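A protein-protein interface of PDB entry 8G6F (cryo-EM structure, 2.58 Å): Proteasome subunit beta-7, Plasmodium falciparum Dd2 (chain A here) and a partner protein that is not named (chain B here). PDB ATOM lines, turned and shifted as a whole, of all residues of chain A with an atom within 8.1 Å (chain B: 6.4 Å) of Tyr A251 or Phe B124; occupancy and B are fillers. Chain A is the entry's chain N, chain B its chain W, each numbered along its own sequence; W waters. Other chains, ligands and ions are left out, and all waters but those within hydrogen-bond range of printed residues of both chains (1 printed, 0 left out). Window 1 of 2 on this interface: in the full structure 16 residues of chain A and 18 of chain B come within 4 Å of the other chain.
The guanidinium group (NH2) of Arg A216 lies within hydrogen-bond range of the side-chain sulfur (SD) of Met B135 (3.8 Å).
The side-chain carboxylate (OE2) of Glu B139 is in salt-bridge range of the guanidinium group (NE) of Arg A216.
The side-chain carboxylate (OE1) of Glu B139 lies within hydrogen-bond range of the side-chain amide nitrogen (ND2) of Asn A247 (3.5 Å).
The backbone carbonyl oxygen (O) of Val B7 lies within hydrogen-bond range of the side-chain hydroxyl (OH) of Tyr B142 (3.5 Å).
OD2 of Asp A250 is in hydrogen-bond range of OG of Ser A248 (3.1 Å).
The backbone NH (N) of Val B7 lies within hydrogen-bond range of the backbone carbonyl oxygen (O) of Pro B123, at 2.9 Å.
Among the printed residues, merely in contact across the chains: Tyr A251 with Phe B124 (3.4 Å), Ser A248 with Pro B123 (3.6 Å), Tyr A251 with Pro B123 (3.7 Å), Asn A247 with Phe B124 (3.8 Å), Asp A250 with Pro B123 (3.8 Å), Ser A248 with Tyr B142 (3.8 Å) and Asn A247 with Tyr B142 (3.8 Å).
Of chain B, only Pro B123 and Phe B124 come within 4 Å of Tyr A251.
Of chain A, only Asn A247 and Tyr A251 come within 4 Å of Phe B124.
Of the printed residues of chain B, Asn A247 touches Phe B124, Glu B139 and Tyr B142.
Printed residues of chain B within 4 Å of Asp A250: Pro B123 (3.8 Å).
Printed residues of chain A within 4 Å of Met B135: Arg A216.
Of the printed residues of chain B, Ser A248 touches Pro B123 (3.6 Å) and Tyr B142 (3.8 Å).
Val A252 touches none of the printed residues of chain B.
The nearest residue of chain A that does not touch Phe B124 is Arg A216 (4.2 Å).
The nearest printed residue of chain A that does not touch Met B135 is Asn A247 (7.3 Å).
Hydrophobic or aromatic side chains of chain B within 4 Å of the printed part of chain A: Pro B123, Phe B124, Met B135 and Tyr B142.
Of the 13 printed residues of chain A, 5 touch a printed residue of chain B.
Printed residues of chain A that touch a printed residue of chain B: Arg A216, Asn A247, Ser A248, Asp A250 and Tyr A251.
Hydrophobic or aromatic side chains of chain A within 4 Å of the printed part of chain B: Tyr A251.
Water W1 lies within hydrogen-bond range of the side-chain hydroxyl (OH) of Tyr A251 (2.6 Å) and the backbone carbonyl oxygen (O) of Phe B124 (2.8 Å).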
ATOM      1  N   PHE A 215      -7.376 -28.365  -4.348  1.00  0.00           N
ATOM      2  CA  PHE A 215      -8.823 -28.542  -4.310  1.00  0.00           C
ATOM      3  C   PHE A 215      -9.244 -29.823  -3.604  1.00  0.00           C
ATOM      4  O   PHE A 215     -10.293 -29.837  -2.954  1.00  0.00           O
ATOM      5  CB  PHE A 215      -9.396 -28.515  -5.726  1.00  0.00           C
ATOM      6  CG  PHE A 215      -9.661 -27.133  -6.242  1.00  0.00           C
ATOM      7  CD1 PHE A 215     -10.337 -26.206  -5.468  1.00  0.00           C
ATOM      8  CD2 PHE A 215      -9.231 -26.758  -7.497  1.00  0.00           C
ATOM      9  CE1 PHE A 215     -10.572 -24.939  -5.935  1.00  0.00           C
ATOM     10  CE2 PHE A 215      -9.469 -25.488  -7.969  1.00  0.00           C
ATOM     11  CZ  PHE A 215     -10.142 -24.581  -7.187  1.00  0.00           C
ATOM     12  N   ARG A 216      -8.463 -30.897  -3.699  1.00  0.00           N
ATOM     13  CA  ARG A 216      -8.915 -32.205  -3.238  1.00  0.00           C
ATOM     14  C   ARG A 216      -8.164 -32.747  -2.030  1.00  0.00           C
ATOM     15  O   ARG A 216      -8.454 -33.865  -1.598  1.00  0.00           O
ATOM     16  CB  ARG A 216      -8.815 -33.221  -4.381  1.00  0.00           C
ATOM     17  CG  ARG A 216      -9.937 -33.153  -5.398  1.00  0.00           C
ATOM     18  CD  ARG A 216     -11.300 -33.434  -4.798  1.00  0.00           C
ATOM     19  NE  ARG A 216     -12.367 -33.074  -5.718  1.00  0.00           N
ATOM     20  CZ  ARG A 216     -13.656 -33.263  -5.480  1.00  0.00           C
ATOM     21  NH1 ARG A 216     -14.079 -33.794  -4.347  1.00  0.00           N
ATOM     22  NH2 ARG A 216     -14.543 -32.907  -6.403  1.00  0.00           N
ATOM     23  N   VAL A 245      -9.410 -21.160  -8.735  1.00  0.00           N
ATOM     24  CA  VAL A 245     -10.826 -20.835  -8.819  1.00  0.00           C
ATOM     25  C   VAL A 245     -11.600 -22.116  -9.086  1.00  0.00           C
ATOM     26  O   VAL A 245     -11.090 -23.059  -9.699  1.00  0.00           O
ATOM     27  CB  VAL A 245     -11.108 -19.787  -9.917  1.00  0.00           C
ATOM     28  CG1 VAL A 245     -10.201 -18.587  -9.748  1.00  0.00           C
ATOM     29  CG2 VAL A 245     -10.941 -20.394 -11.296  1.00  0.00           C
ATOM     30  N   LEU A 246     -12.842 -22.149  -8.614  1.00  0.00           N
ATOM     31  CA  LEU A 246     -13.695 -23.303  -8.840  1.00  0.00           C
ATOM     32  C   LEU A 246     -14.039 -23.433 -10.318  1.00  0.00           C
ATOM     33  O   LEU A 246     -14.126 -22.444 -11.048  1.00  0.00           O
ATOM     34  CB  LEU A 246     -14.970 -23.192  -8.009  1.00  0.00           C
ATOM     35  CG  LEU A 246     -14.747 -23.326  -6.505  1.00  0.00           C
ATOM     36  CD1 LEU A 246     -15.900 -22.714  -5.738  1.00  0.00           C
ATOM     37  CD2 LEU A 246     -14.556 -24.781  -6.122  1.00  0.00           C
ATOM     38  N   ASN A 247     -14.239 -24.673 -10.756  1.00  0.00           N
ATOM     39  CA  ASN A 247     -14.437 -24.979 -12.164  1.00  0.00           C
ATOM     40  C   ASN A 247     -15.899 -25.194 -12.525  1.00  0.00           C
ATOM     41  O   ASN A 247     -16.186 -25.704 -13.612  1.00  0.00           O
ATOM     42  CB  ASN A 247     -13.618 -26.213 -12.558  1.00  0.00           C
ATOM     43  CG  ASN A 247     -13.738 -27.345 -11.559  1.00  0.00           C
ATOM     44  OD1 ASN A 247     -14.234 -27.159 -10.452  1.00  0.00           O
ATOM     45  ND2 ASN A 247     -13.284 -28.526 -11.948  1.00  0.00           N
ATOM     46  N   SER A 248     -16.828 -24.820 -11.649  1.00  0.00           N
ATOM     47  CA  SER A 248     -18.246 -24.973 -11.933  1.00  0.00           C
ATOM     48  C   SER A 248     -19.026 -23.849 -11.268  1.00  0.00           C
ATOM     49  O   SER A 248     -18.672 -23.401 -10.175  1.00  0.00           O
ATOM     50  CB  SER A 248     -18.764 -26.328 -11.450  1.00  0.00           C
ATOM     51  OG  SER A 248     -19.946 -26.687 -12.134  1.00  0.00           O
ATOM     52  N   ALA A 249     -20.083 -23.396 -11.938  1.00  0.00           N
ATOM     53  CA  ALA A 249     -21.019 -22.440 -11.365  1.00  0.00           C
ATOM     54  C   ALA A 249     -22.121 -23.109 -10.556  1.00  0.00           C
ATOM     55  O   ALA A 249     -22.822 -22.424  -9.798  1.00  0.00           O
ATOM     56  CB  ALA A 249     -21.644 -21.594 -12.475  1.00  0.00           C
ATOM     57  N   ASP A 250     -22.289 -24.424 -10.695  1.00  0.00           N
ATOM     58  CA  ASP A 250     -23.233 -25.141  -9.853  1.00  0.00           C
ATOM     59  C   ASP A 250     -22.806 -25.111  -8.395  1.00  0.00           C
ATOM     60  O   ASP A 250     -23.656 -25.176  -7.500  1.00  0.00           O
ATOM     61  CB  ASP A 250     -23.377 -26.579 -10.339  1.00  0.00           C
ATOM     62  CG  ASP A 250     -23.810 -26.657 -11.783  1.00  0.00           C
ATOM     63  OD1 ASP A 250     -24.976 -26.316 -12.072  1.00  0.00           O
ATOM     64  OD2 ASP A 250     -22.988 -27.057 -12.632  1.00  0.00           O
ATOM     65  N   TYR A 251     -21.503 -25.015  -8.135  1.00  0.00           N
ATOM     66  CA  TYR A 251     -21.039 -24.812  -6.769  1.00  0.00           C
ATOM     67  C   TYR A 251     -21.588 -23.514  -6.198  1.00  0.00           C
ATOM     68  O   TYR A 251     -22.068 -23.471  -5.061  1.00  0.00           O
ATOM     69  CB  TYR A 251     -19.515 -24.783  -6.733  1.00  0.00           C
ATOM     70  CG  TYR A 251     -18.839 -26.041  -7.204  1.00  0.00           C
ATOM     71  CD1 TYR A 251     -19.309 -27.291  -6.834  1.00  0.00           C
ATOM     72  CD2 TYR A 251     -17.711 -25.977  -8.004  1.00  0.00           C
ATOM     73  CE1 TYR A 251     -18.681 -28.434  -7.257  1.00  0.00           C
ATOM     74  CE2 TYR A 251     -17.082 -27.114  -8.432  1.00  0.00           C
ATOM     75  CZ  TYR A 251     -17.568 -28.339  -8.057  1.00  0.00           C
ATOM     76  OH  TYR A 251     -16.934 -29.477  -8.487  1.00  0.00           O
ATOM     77  N   VAL A 252     -21.522 -22.439  -6.983  1.00  0.00           N
ATOM     78  CA  VAL A 252     -21.880 -21.116  -6.494  1.00  0.00           C
ATOM     79  C   VAL A 252     -23.384 -20.892  -6.503  1.00  0.00           C
ATOM     80  O   VAL A 252     -23.869 -19.976  -5.830  1.00  0.00           O
ATOM     81  CB  VAL A 252     -21.176 -20.043  -7.339  1.00  0.00           C
ATOM     82  CG1 VAL A 252     -21.259 -18.692  -6.670  1.00  0.00           C
ATOM     83  CG2 VAL A 252     -19.730 -20.425  -7.575  1.00  0.00           C
ATOM     84  N   TYR A 253     -24.130 -21.701  -7.242  1.00  0.00           N
ATOM     85  CA  TYR A 253     -25.572 -21.531  -7.311  1.00  0.00           C
ATOM     86  C   TYR A 253     -26.168 -21.507  -5.902  1.00  0.00           C
ATOM     87  O   TYR A 253     -25.915 -22.428  -5.114  1.00  0.00           O
ATOM     88  CB  TYR A 253     -26.182 -22.671  -8.122  1.00  0.00           C
ATOM     89  CG  TYR A 253     -27.587 -22.421  -8.609  1.00  0.00           C
ATOM     90  CD1 TYR A 253     -27.872 -21.375  -9.471  1.00  0.00           C
ATOM     91  CD2 TYR A 253     -28.627 -23.248  -8.216  1.00  0.00           C
ATOM     92  CE1 TYR A 253     -29.155 -21.156  -9.920  1.00  0.00           C
ATOM     93  CE2 TYR A 253     -29.908 -23.037  -8.662  1.00  0.00           C
ATOM     94  CZ  TYR A 253     -30.168 -21.990  -9.512  1.00  0.00           C
ATOM     95  OH  TYR A 253     -31.454 -21.783  -9.953  1.00  0.00           O
ATOM     96  N   PRO A 254     -26.954 -20.487  -5.546  1.00  0.00           N
ATOM     97  CA  PRO A 254     -27.525 -20.438  -4.194  1.00  0.00           C
ATOM     98  C   PRO A 254     -28.412 -21.637  -3.897  1.00  0.00           C
ATOM     99  O   PRO A 254     -29.101 -22.164  -4.771  1.00  0.00           O
ATOM    100  CB  PRO A 254     -28.333 -19.136  -4.195  1.00  0.00           C
ATOM    101  CG  PRO A 254     -27.731 -18.313  -5.252  1.00  0.00           C
ATOM    102  CD  PRO A 254     -27.238 -19.254  -6.299  1.00  0.00           C
ATOM    103  N   SER A 255     -28.384 -22.065  -2.635  1.00  0.00           N
ATOM    104  CA  SER A 255     -29.170 -23.225  -2.228  1.00  0.00           C
ATOM    105  C   SER A 255     -30.660 -22.919  -2.215  1.00  0.00           C
ATOM    106  O   SER A 255     -31.475 -23.817  -2.443  1.00  0.00           O
ATOM    107  CB  SER A 255     -28.723 -23.705  -0.851  1.00  0.00           C
ATOM    108  OG  SER A 255     -27.314 -23.724  -0.754  1.00  0.00           O
ATOM    109  N   GLY B   5     -19.355 -39.819 -13.014  1.00  0.00           N
ATOM    110  CA  GLY B   5     -20.463 -39.203 -13.710  1.00  0.00           C
ATOM    111  C   GLY B   5     -20.224 -37.718 -13.843  1.00  0.00           C
ATOM    112  O   GLY B   5     -19.479 -37.117 -13.067  1.00  0.00           O
ATOM    113  N   LEU B   6     -20.863 -37.135 -14.850  1.00  0.00           N
ATOM    114  CA  LEU B   6     -20.820 -35.692 -15.018  1.00  0.00           C
ATOM    115  C   LEU B   6     -22.094 -35.220 -15.695  1.00  0.00           C
ATOM    116  O   LEU B   6     -22.840 -36.002 -16.287  1.00  0.00           O
ATOM    117  CB  LEU B   6     -19.584 -35.240 -15.808  1.00  0.00           C
ATOM    118  CG  LEU B   6     -19.384 -35.682 -17.254  1.00  0.00           C
ATOM    119  CD1 LEU B   6     -20.098 -34.775 -18.228  1.00  0.00           C
ATOM    120  CD2 LEU B   6     -17.906 -35.698 -17.556  1.00  0.00           C
ATOM    121  N   VAL B   7     -22.333 -33.918 -15.582  1.00  0.00           N
ATOM    122  CA  VAL B   7     -23.493 -33.258 -16.165  1.00  0.00           C
ATOM    123  C   VAL B   7     -23.010 -32.411 -17.330  1.00  0.00           C
ATOM    124  O   VAL B   7     -22.113 -31.576 -17.168  1.00  0.00           O
ATOM    125  CB  VAL B   7     -24.230 -32.394 -15.127  1.00  0.00           C
ATOM    126  CG1 VAL B   7     -25.351 -31.621 -15.780  1.00  0.00           C
ATOM    127  CG2 VAL B   7     -24.768 -33.248 -14.003  1.00  0.00           C
ATOM    128  N   LEU B 110     -27.016 -35.092 -10.923  1.00  0.00           N
ATOM    129  CA  LEU B 110     -26.025 -36.094 -10.579  1.00  0.00           C
ATOM    130  C   LEU B 110     -25.844 -36.083  -9.072  1.00  0.00           C
ATOM    131  O   LEU B 110     -25.671 -35.018  -8.473  1.00  0.00           O
ATOM    132  CB  LEU B 110     -24.697 -35.817 -11.287  1.00  0.00           C
ATOM    133  CG  LEU B 110     -23.617 -36.885 -11.140  1.00  0.00           C
ATOM    134  CD1 LEU B 110     -23.967 -38.103 -11.958  1.00  0.00           C
ATOM    135  CD2 LEU B 110     -22.280 -36.332 -11.552  1.00  0.00           C
ATOM    136  N   LEU B 121     -25.466 -33.426  -4.303  1.00  0.00           N
ATOM    137  CA  LEU B 121     -25.730 -33.075  -5.691  1.00  0.00           C
ATOM    138  C   LEU B 121     -24.495 -32.395  -6.268  1.00  0.00           C
ATOM    139  O   LEU B 121     -24.046 -31.373  -5.745  1.00  0.00           O
ATOM    140  CB  LEU B 121     -26.950 -32.163  -5.780  1.00  0.00           C
ATOM    141  CG  LEU B 121     -27.358 -31.650  -7.158  1.00  0.00           C
ATOM    142  CD1 LEU B 121     -28.164 -32.687  -7.903  1.00  0.00           C
ATOM    143  CD2 LEU B 121     -28.147 -30.366  -7.015  1.00  0.00           C
ATOM    144  N   LEU B 122     -23.957 -32.953  -7.343  1.00  0.00           N
ATOM    145  CA  LEU B 122     -22.666 -32.560  -7.881  1.00  0.00           C
ATOM    146  C   LEU B 122     -22.751 -32.316  -9.377  1.00  0.00           C
ATOM    147  O   LEU B 122     -23.639 -32.845 -10.051  1.00  0.00           O
ATOM    148  CB  LEU B 122     -21.613 -33.643  -7.607  1.00  0.00           C
ATOM    149  CG  LEU B 122     -21.414 -34.030  -6.146  1.00  0.00           C
ATOM    150  CD1 LEU B 122     -20.502 -35.220  -6.040  1.00  0.00           C
ATOM    151  CD2 LEU B 122     -20.855 -32.867  -5.370  1.00  0.00           C
ATOM    152  N   PRO B 123     -21.845 -31.499  -9.929  1.00  0.00           N
ATOM    153  CA  PRO B 123     -21.726 -31.416 -11.390  1.00  0.00           C
ATOM    154  C   PRO B 123     -20.969 -32.599 -11.967  1.00  0.00           C
ATOM    155  O   PRO B 123     -21.252 -33.048 -13.080  1.00  0.00           O
ATOM    156  CB  PRO B 123     -20.972 -30.100 -11.604  1.00  0.00           C
ATOM    157  CG  PRO B 123     -20.200 -29.910 -10.367  1.00  0.00           C
ATOM    158  CD  PRO B 123     -21.014 -30.488  -9.255  1.00  0.00           C
ATOM    159  N   PHE B 124     -19.996 -33.103 -11.216  1.00  0.00           N
ATOM    160  CA  PHE B 124     -19.287 -34.318 -11.583  1.00  0.00           C
ATOM    161  C   PHE B 124     -18.831 -35.006 -10.308  1.00  0.00           C
ATOM    162  O   PHE B 124     -18.696 -34.379  -9.258  1.00  0.00           O
ATOM    163  CB  PHE B 124     -18.095 -34.030 -12.506  1.00  0.00           C
ATOM    164  CG  PHE B 124     -17.036 -33.170 -11.884  1.00  0.00           C
ATOM    165  CD1 PHE B 124     -17.087 -31.797 -11.997  1.00  0.00           C
ATOM    166  CD2 PHE B 124     -15.988 -33.737 -11.186  1.00  0.00           C
ATOM    167  CE1 PHE B 124     -16.120 -31.010 -11.426  1.00  0.00           C
ATOM    168  CE2 PHE B 124     -15.020 -32.952 -10.613  1.00  0.00           C
ATOM    169  CZ  PHE B 124     -15.085 -31.589 -10.732  1.00  0.00           C
ATOM    170  N   THR B 125     -18.600 -36.312 -10.410  1.00  0.00           N
ATOM    171  CA  THR B 125     -18.135 -37.086  -9.266  1.00  0.00           C
ATOM    172  C   THR B 125     -17.482 -38.369  -9.755  1.00  0.00           C
ATOM    173  O   THR B 125     -17.651 -38.773 -10.905  1.00  0.00           O
ATOM    174  CB  THR B 125     -19.281 -37.405  -8.296  1.00  0.00           C
ATOM    175  OG1 THR B 125     -18.743 -37.737  -7.010  1.00  0.00           O
ATOM    176  CG2 THR B 125     -20.123 -38.563  -8.800  1.00  0.00           C
ATOM    177  N   ALA B 126     -16.727 -38.997  -8.856  1.00  0.00           N
ATOM    178  CA  ALA B 126     -16.106 -40.287  -9.113  1.00  0.00           C
ATOM    179  C   ALA B 126     -16.040 -41.069  -7.811  1.00  0.00           C
ATOM    180  O   ALA B 126     -15.817 -40.492  -6.746  1.00  0.00           O
ATOM    181  CB  ALA B 126     -14.704 -40.130  -9.708  1.00  0.00           C
ATOM    182  N   MET B 135     -10.900 -38.524 -10.496  1.00  0.00           N
ATOM    183  CA  MET B 135     -11.157 -37.171 -10.035  1.00  0.00           C
ATOM    184  C   MET B 135     -10.059 -36.219 -10.463  1.00  0.00           C
ATOM    185  O   MET B 135     -10.333 -35.048 -10.725  1.00  0.00           O
ATOM    186  CB  MET B 135     -11.298 -37.154  -8.516  1.00  0.00           C
ATOM    187  CG  MET B 135     -12.068 -35.964  -7.989  1.00  0.00           C
ATOM    188  SD  MET B 135     -13.849 -36.203  -8.102  1.00  0.00           S
ATOM    189  CE  MET B 135     -14.147 -37.110  -6.590  1.00  0.00           C
ATOM    190  N   LEU B 138     -11.042 -35.412 -13.988  1.00  0.00           N
ATOM    191  CA  LEU B 138     -12.241 -34.580 -14.034  1.00  0.00           C
ATOM    192  C   LEU B 138     -11.955 -33.162 -13.561  1.00  0.00           C
ATOM    193  O   LEU B 138     -12.425 -32.194 -14.165  1.00  0.00           O
ATOM    194  CB  LEU B 138     -13.344 -35.209 -13.188  1.00  0.00           C
ATOM    195  CG  LEU B 138     -13.929 -36.517 -13.715  1.00  0.00           C
ATOM    196  CD1 LEU B 138     -14.733 -37.212 -12.633  1.00  0.00           C
ATOM    197  CD2 LEU B 138     -14.783 -36.262 -14.939  1.00  0.00           C
ATOM    198  N   GLU B 139     -11.198 -33.014 -12.477  1.00  0.00           N
ATOM    199  CA  GLU B 139     -10.849 -31.687 -11.993  1.00  0.00           C
ATOM    200  C   GLU B 139     -10.018 -30.938 -13.020  1.00  0.00           C
ATOM    201  O   GLU B 139     -10.200 -29.732 -13.216  1.00  0.00           O
ATOM    202  CB  GLU B 139     -10.087 -31.796 -10.676  1.00  0.00           C
ATOM    203  CG  GLU B 139     -10.915 -32.317  -9.531  1.00  0.00           C
ATOM    204  CD  GLU B 139     -11.668 -31.223  -8.818  1.00  0.00           C
ATOM    205  OE1 GLU B 139     -11.662 -30.078  -9.310  1.00  0.00           O
ATOM    206  OE2 GLU B 139     -12.268 -31.506  -7.764  1.00  0.00           O
ATOM    207  N   TYR B 142     -12.791 -30.638 -16.545  1.00  0.00           N
ATOM    208  CA  TYR B 142     -14.226 -30.393 -16.561  1.00  0.00           C
ATOM    209  C   TYR B 142     -14.537 -28.914 -16.750  1.00  0.00           C
ATOM    210  O   TYR B 142     -13.835 -28.044 -16.229  1.00  0.00           O
ATOM    211  CB  TYR B 142     -14.870 -30.890 -15.267  1.00  0.00           C
ATOM    212  CG  TYR B 142     -16.341 -30.553 -15.160  1.00  0.00           C
ATOM    213  CD1 TYR B 142     -17.307 -31.405 -15.670  1.00  0.00           C
ATOM    214  CD2 TYR B 142     -16.762 -29.376 -14.556  1.00  0.00           C
ATOM    215  CE1 TYR B 142     -18.642 -31.098 -15.577  1.00  0.00           C
ATOM    216  CE2 TYR B 142     -18.095 -29.063 -14.463  1.00  0.00           C
ATOM    217  CZ  TYR B 142     -19.030 -29.925 -14.974  1.00  0.00           C
ATOM    218  OH  TYR B 142     -20.362 -29.609 -14.878  1.00  0.00           O
HETATM  219  O   HOH W   1     -17.787 -31.944  -8.105  1.00  0.00           O
